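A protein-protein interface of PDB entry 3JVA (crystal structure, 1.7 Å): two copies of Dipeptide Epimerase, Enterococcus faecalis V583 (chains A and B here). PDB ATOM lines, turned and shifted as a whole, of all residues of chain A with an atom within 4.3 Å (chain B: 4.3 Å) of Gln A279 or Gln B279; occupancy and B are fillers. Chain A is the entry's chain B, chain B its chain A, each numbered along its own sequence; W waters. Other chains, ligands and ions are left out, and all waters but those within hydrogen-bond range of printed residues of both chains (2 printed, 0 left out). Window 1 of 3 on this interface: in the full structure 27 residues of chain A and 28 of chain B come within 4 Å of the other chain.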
ATOM      1  N   LEU A 275       3.721  -6.625 -13.301  1.00  0.00           N
ATOM      2  CA  LEU A 275       2.326  -7.012 -13.155  1.00  0.00           C
ATOM      3  C   LEU A 275       1.602  -6.928 -14.497  1.00  0.00           C
ATOM      4  O   LEU A 275       0.792  -7.797 -14.824  1.00  0.00           O
ATOM      5  CB  LEU A 275       1.632  -6.122 -12.121  1.00  0.00           C
ATOM      6  CG  LEU A 275       1.963  -6.469 -10.668  1.00  0.00           C
ATOM      7  CD1 LEU A 275       1.484  -5.338  -9.755  1.00  0.00           C
ATOM      8  CD2 LEU A 275       1.317  -7.796 -10.292  1.00  0.00           C
ATOM      9  N   LYS A 276       1.901  -5.892 -15.276  1.00  0.00           N
ATOM     10  CA  LYS A 276       1.274  -5.722 -16.586  1.00  0.00           C
ATOM     11  C   LYS A 276       1.655  -6.879 -17.495  1.00  0.00           C
ATOM     12  O   LYS A 276       0.812  -7.445 -18.192  1.00  0.00           O
ATOM     13  CB  LYS A 276       1.731  -4.419 -17.241  1.00  0.00           C
ATOM     14  CG  LYS A 276       1.302  -3.151 -16.519  1.00  0.00           C
ATOM     15  CD  LYS A 276       1.810  -1.944 -17.282  1.00  0.00           C
ATOM     16  CE  LYS A 276       1.495  -0.642 -16.576  1.00  0.00           C
ATOM     17  NZ  LYS A 276       2.152   0.490 -17.292  1.00  0.00           N
ATOM     18  N   ILE A 277       2.941  -7.213 -17.500  1.00  0.00           N
ATOM     19  CA  ILE A 277       3.412  -8.314 -18.330  1.00  0.00           C
ATOM     20  C   ILE A 277       2.672  -9.601 -17.982  1.00  0.00           C
ATOM     21  O   ILE A 277       2.161 -10.291 -18.860  1.00  0.00           O
ATOM     22  CB  ILE A 277       4.935  -8.545 -18.154  1.00  0.00           C
ATOM     23  CG1 ILE A 277       5.709  -7.345 -18.716  1.00  0.00           C
ATOM     24  CG2 ILE A 277       5.349  -9.833 -18.876  1.00  0.00           C
ATOM     25  CD1 ILE A 277       7.195  -7.333 -18.369  1.00  0.00           C
ATOM     26  N   ASN A 278       2.603  -9.922 -16.694  1.00  0.00           N
ATOM     27  CA  ASN A 278       1.923 -11.139 -16.287  1.00  0.00           C
ATOM     28  C   ASN A 278       0.431 -11.164 -16.629  1.00  0.00           C
ATOM     29  O   ASN A 278      -0.086 -12.198 -17.046  1.00  0.00           O
ATOM     30  CB  ASN A 278       2.106 -11.387 -14.792  1.00  0.00           C
ATOM     31  CG  ASN A 278       1.553 -12.725 -14.370  1.00  0.00           C
ATOM     32  OD1 ASN A 278       1.926 -13.756 -14.927  1.00  0.00           O
ATOM     33  ND2 ASN A 278       0.650 -12.722 -13.392  1.00  0.00           N
ATOM     34  N   GLN A 279      -0.262 -10.040 -16.450  1.00  0.00           N
ATOM     35  CA  GLN A 279      -1.692  -9.987 -16.762  1.00  0.00           C
ATOM     36  C   GLN A 279      -1.926 -10.130 -18.260  1.00  0.00           C
ATOM     37  O   GLN A 279      -2.898 -10.749 -18.688  1.00  0.00           O
ATOM     38  CB  GLN A 279      -2.308  -8.669 -16.285  1.00  0.00           C
ATOM     39  CG  GLN A 279      -2.223  -8.448 -14.789  1.00  0.00           C
ATOM     40  CD  GLN A 279      -2.697  -7.060 -14.394  1.00  0.00           C
ATOM     41  OE1 GLN A 279      -2.512  -6.091 -15.141  1.00  0.00           O
ATOM     42  NE2 GLN A 279      -3.293  -6.954 -13.217  1.00  0.00           N
ATOM     43  N   ILE A 280      -1.042  -9.542 -19.061  1.00  0.00           N
ATOM     44  CA  ILE A 280      -1.163  -9.647 -20.511  1.00  0.00           C
ATOM     45  C   ILE A 280      -0.967 -11.106 -20.917  1.00  0.00           C
ATOM     46  O   ILE A 280      -1.738 -11.651 -21.714  1.00  0.00           O
ATOM     47  CB  ILE A 280      -0.101  -8.782 -21.224  1.00  0.00           C
ATOM     48  CG1 ILE A 280      -0.454  -7.296 -21.066  1.00  0.00           C
ATOM     49  CG2 ILE A 280      -0.017  -9.169 -22.705  1.00  0.00           C
ATOM     50  CD1 ILE A 280       0.681  -6.342 -21.426  1.00  0.00           C
ATOM     51  N   CYS A 281       0.064 -11.738 -20.361  1.00  0.00           N
ATOM     52  CA  CYS A 281       0.362 -13.134 -20.677  1.00  0.00           C
ATOM     53  C   CYS A 281      -0.752 -14.063 -20.201  1.00  0.00           C
ATOM     54  O   CYS A 281      -1.214 -14.932 -20.944  1.00  0.00           O
ATOM     55  CB  CYS A 281       1.689 -13.549 -20.036  1.00  0.00           C
ATOM     56  SG  CYS A 281       3.152 -12.782 -20.766  1.00  0.00           S
ATOM     57  N   GLU A 282      -1.175 -13.878 -18.954  1.00  0.00           N
ATOM     58  CA  GLU A 282      -2.229 -14.698 -18.379  1.00  0.00           C
ATOM     59  C   GLU A 282      -3.486 -14.633 -19.246  1.00  0.00           C
ATOM     60  O   GLU A 282      -4.118 -15.649 -19.514  1.00  0.00           O
ATOM     61  CB  GLU A 282      -2.529 -14.219 -16.955  1.00  0.00           C
ATOM     62  CG  GLU A 282      -3.598 -15.002 -16.220  1.00  0.00           C
ATOM     63  CD  GLU A 282      -3.690 -14.596 -14.758  1.00  0.00           C
ATOM     64  OE1 GLU A 282      -3.720 -13.381 -14.481  1.00  0.00           O
ATOM     65  OE2 GLU A 282      -3.738 -15.490 -13.891  1.00  0.00           O
ATOM     66  N   THR A 283      -3.834 -13.431 -19.691  1.00  0.00           N
ATOM     67  CA  THR A 283      -5.009 -13.237 -20.530  1.00  0.00           C
ATOM     68  C   THR A 283      -4.863 -13.985 -21.855  1.00  0.00           C
ATOM     69  O   THR A 283      -5.839 -14.521 -22.392  1.00  0.00           O
ATOM     70  CB  THR A 283      -5.231 -11.739 -20.776  1.00  0.00           C
ATOM     71  OG1 THR A 283      -5.446 -11.100 -19.515  1.00  0.00           O
ATOM     72  CG2 THR A 283      -6.439 -11.500 -21.665  1.00  0.00           C
ATOM     73  N   LEU B 275      -8.589  -4.107 -13.610  1.00  0.00           N
ATOM     74  CA  LEU B 275      -7.197  -3.667 -13.631  1.00  0.00           C
ATOM     75  C   LEU B 275      -6.482  -4.284 -14.833  1.00  0.00           C
ATOM     76  O   LEU B 275      -5.662  -3.627 -15.473  1.00  0.00           O
ATOM     77  CB  LEU B 275      -6.486  -4.064 -12.327  1.00  0.00           C
ATOM     78  CG  LEU B 275      -6.861  -3.214 -11.109  1.00  0.00           C
ATOM     79  CD1 LEU B 275      -6.430  -3.922  -9.822  1.00  0.00           C
ATOM     80  CD2 LEU B 275      -6.211  -1.838 -11.226  1.00  0.00           C
ATOM     81  N   LYS B 276      -6.797  -5.542 -15.139  1.00  0.00           N
ATOM     82  CA  LYS B 276      -6.185  -6.218 -16.280  1.00  0.00           C
ATOM     83  C   LYS B 276      -6.559  -5.484 -17.567  1.00  0.00           C
ATOM     84  O   LYS B 276      -5.705  -5.192 -18.402  1.00  0.00           O
ATOM     85  CB  LYS B 276      -6.668  -7.667 -16.388  1.00  0.00           C
ATOM     86  CG  LYS B 276      -6.304  -8.574 -15.220  1.00  0.00           C
ATOM     87  CD  LYS B 276      -6.797  -9.990 -15.524  1.00  0.00           C
ATOM     88  CE  LYS B 276      -6.593 -10.948 -14.362  1.00  0.00           C
ATOM     89  NZ  LYS B 276      -7.180 -12.283 -14.698  1.00  0.00           N
ATOM     90  N   ILE B 277      -7.847  -5.199 -17.727  1.00  0.00           N
ATOM     91  CA  ILE B 277      -8.321  -4.496 -18.921  1.00  0.00           C
ATOM     92  C   ILE B 277      -7.597  -3.168 -19.093  1.00  0.00           C
ATOM     93  O   ILE B 277      -7.069  -2.867 -20.170  1.00  0.00           O
ATOM     94  CB  ILE B 277      -9.843  -4.226 -18.847  1.00  0.00           C
ATOM     95  CG1 ILE B 277     -10.602  -5.550 -18.870  1.00  0.00           C
ATOM     96  CG2 ILE B 277     -10.282  -3.345 -20.022  1.00  0.00           C
ATOM     97  CD1 ILE B 277     -12.086  -5.405 -18.628  1.00  0.00           C
ATOM     98  N   ASN B 278      -7.553  -2.375 -18.029  1.00  0.00           N
ATOM     99  CA  ASN B 278      -6.903  -1.079 -18.114  1.00  0.00           C
ATOM    100  C   ASN B 278      -5.420  -1.178 -18.459  1.00  0.00           C
ATOM    101  O   ASN B 278      -4.921  -0.394 -19.255  1.00  0.00           O
ATOM    102  CB  ASN B 278      -7.076  -0.294 -16.811  1.00  0.00           C
ATOM    103  CG  ASN B 278      -6.524   1.111 -16.912  1.00  0.00           C
ATOM    104  OD1 ASN B 278      -6.927   1.887 -17.788  1.00  0.00           O
ATOM    105  ND2 ASN B 278      -5.592   1.452 -16.024  1.00  0.00           N
ATOM    106  N   GLN B 279      -4.715  -2.146 -17.883  1.00  0.00           N
ATOM    107  CA  GLN B 279      -3.291  -2.270 -18.168  1.00  0.00           C
ATOM    108  C   GLN B 279      -3.018  -2.776 -19.582  1.00  0.00           C
ATOM    109  O   GLN B 279      -2.017  -2.400 -20.196  1.00  0.00           O
ATOM    110  CB  GLN B 279      -2.623  -3.146 -17.103  1.00  0.00           C
ATOM    111  CG  GLN B 279      -2.866  -2.564 -15.712  1.00  0.00           C
ATOM    112  CD  GLN B 279      -1.771  -2.876 -14.719  1.00  0.00           C
ATOM    113  OE1 GLN B 279      -1.543  -4.032 -14.364  1.00  0.00           O
ATOM    114  NE2 GLN B 279      -1.086  -1.834 -14.258  1.00  0.00           N
ATOM    115  N   ILE B 280      -3.908  -3.614 -20.106  1.00  0.00           N
ATOM    116  CA  ILE B 280      -3.756  -4.116 -21.470  1.00  0.00           C
ATOM    117  C   ILE B 280      -3.958  -2.917 -22.401  1.00  0.00           C
ATOM    118  O   ILE B 280      -3.177  -2.682 -23.334  1.00  0.00           O
ATOM    119  CB  ILE B 280      -4.815  -5.198 -21.776  1.00  0.00           C
ATOM    120  CG1 ILE B 280      -4.465  -6.481 -21.019  1.00  0.00           C
ATOM    121  CG2 ILE B 280      -4.905  -5.456 -23.284  1.00  0.00           C
ATOM    122  CD1 ILE B 280      -5.542  -7.538 -21.087  1.00  0.00           C
ATOM    123  N   CYS B 281      -5.002  -2.145 -22.123  1.00  0.00           N
ATOM    124  CA  CYS B 281      -5.307  -0.964 -22.933  1.00  0.00           C
ATOM    125  C   CYS B 281      -4.194   0.076 -22.879  1.00  0.00           C
ATOM    126  O   CYS B 281      -3.752   0.582 -23.912  1.00  0.00           O
ATOM    127  CB  CYS B 281      -6.616  -0.331 -22.461  1.00  0.00           C
ATOM    128  SG  CYS B 281      -8.074  -1.278 -22.906  1.00  0.00           S
ATOM    129  N   GLU B 282      -3.757   0.400 -21.667  1.00  0.00           N
ATOM    130  CA  GLU B 282      -2.700   1.381 -21.456  1.00  0.00           C
ATOM    131  C   GLU B 282      -1.441   0.999 -22.227  1.00  0.00           C
ATOM    132  O   GLU B 282      -0.767   1.850 -22.805  1.00  0.00           O
ATOM    133  CB  GLU B 282      -2.404   1.476 -19.960  1.00  0.00           C
ATOM    134  CG  GLU B 282      -1.354   2.485 -19.563  1.00  0.00           C
ATOM    135  CD  GLU B 282      -1.208   2.557 -18.059  1.00  0.00           C
ATOM    136  OE1 GLU B 282      -1.127   1.481 -17.433  1.00  0.00           O
ATOM    137  OE2 GLU B 282      -1.172   3.676 -17.507  1.00  0.00           O
ATOM    138  N   THR B 283      -1.131  -0.290 -22.238  1.00  0.00           N
ATOM    139  CA  THR B 283       0.048  -0.774 -22.947  1.00  0.00           C
ATOM    140  C   THR B 283      -0.076  -0.530 -24.459  1.00  0.00           C
ATOM    141  O   THR B 283       0.922  -0.276 -25.144  1.00  0.00           O
ATOM    142  CB  THR B 283       0.250  -2.271 -22.668  1.00  0.00           C
ATOM    143  OG1 THR B 283       0.440  -2.460 -21.257  1.00  0.00           O
ATOM    144  CG2 THR B 283       1.470  -2.802 -23.418  1.00  0.00           C
HETATM  145  O   HOH W   1      -6.720 -12.855 -17.704  1.00  0.00           O
HETATM  146  O   HOH W   2       1.700   0.091 -20.184  1.00  0.00           O
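OE1 of Gln B279 lies close to OE1 of Gln A279, at 2.4 Å. The side-chain carboxylate (OE1) of Glu B282 is in salt-bridge range of the side-chain amino group (NZ) of Lys A276 (3.4 Å). The side-chain carboxylate (OE1) of Glu A282 lies within salt-bridge range of the side-chain amino group (NZ) of Lys B276 (3.6 Å).
OG1 of Thr A283 lies within hydrogen-bond range of O of Gln A279 (2.7 Å). The backbone carbonyl oxygen (O) of Gln B279 is in hydrogen-bond range of the side-chain hydroxyl (OG1) of Thr B283, 2.7 Å away.
Lys A276 touches Gln B279. Gln A279 touches Lys B276 (OE1 to CA, 3.8 Å). Ile A280 touches Thr B283 (CD1 to OG1, 3.9 Å). OG1 of Thr A283 touches CD1 of Ile B280, 3.9 Å away.
Of the printed residues of chain B, Lys A276 touches Gln B279 (3.5 Å) and Glu B282 (3.4 Å). Of the printed residues of chain B, Gln A279 touches Lys B276 (3.8 Å) and Gln B279 (2.4 Å). Of the printed residues of chain B, Ile A280 touches Thr B283 (3.9 Å). Gln B279 touches just these residues of chain A: Lys A276 and Gln A279. The nearest printed residue of chain B that does not touch Gln A279 is Leu B275 (4.01 Å). The nearest printed residue of chain A that does not touch Gln B279 is Leu A275 (4.3 Å).
Of the 9 printed residues of chain A, 5 touch a printed residue of chain B. Printed residues of chain A that touch a printed residue of chain B: Lys A276, Gln A279, Ile A280, Glu A282 and Thr A283. Hydrophobic or aromatic side chains of chain A that line the printed part of chain B: Ile A280. Of the 9 printed residues of chain B, 5 touch a printed residue of chain A. Printed residues of chain B that touch a printed residue of chain A: Lys B276, Gln B279, Ile B280, Glu B282 and Thr B283. Hydrophobic or aromatic side chains of chain B that line the printed part of chain A: Ile B280.
Lys A276 touches Gln B279, and with the chains exchanged Gln A279 touches Lys B276. Lys A276 touches Glu B282, and with the chains exchanged Glu A282 touches Lys B276. Gln B279 touches its own counterpart, Gln A279. Ile A280 touches Thr B283, and with the chains exchanged Thr A283 touches Ile B280. 9 positions are printed for both chains. Of the 7 pairs that touch across the chains among the printed residues, 7 have their exchanged pair printed and touching as well.
Water W1 bridges the side-chain hydroxyl of Thr A283 (2.8 Å) and the side-chain amino group of Lys B276 (3.1 Å). Water W2 bridges NZ of Lys A276 and OG1 of Thr B283.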
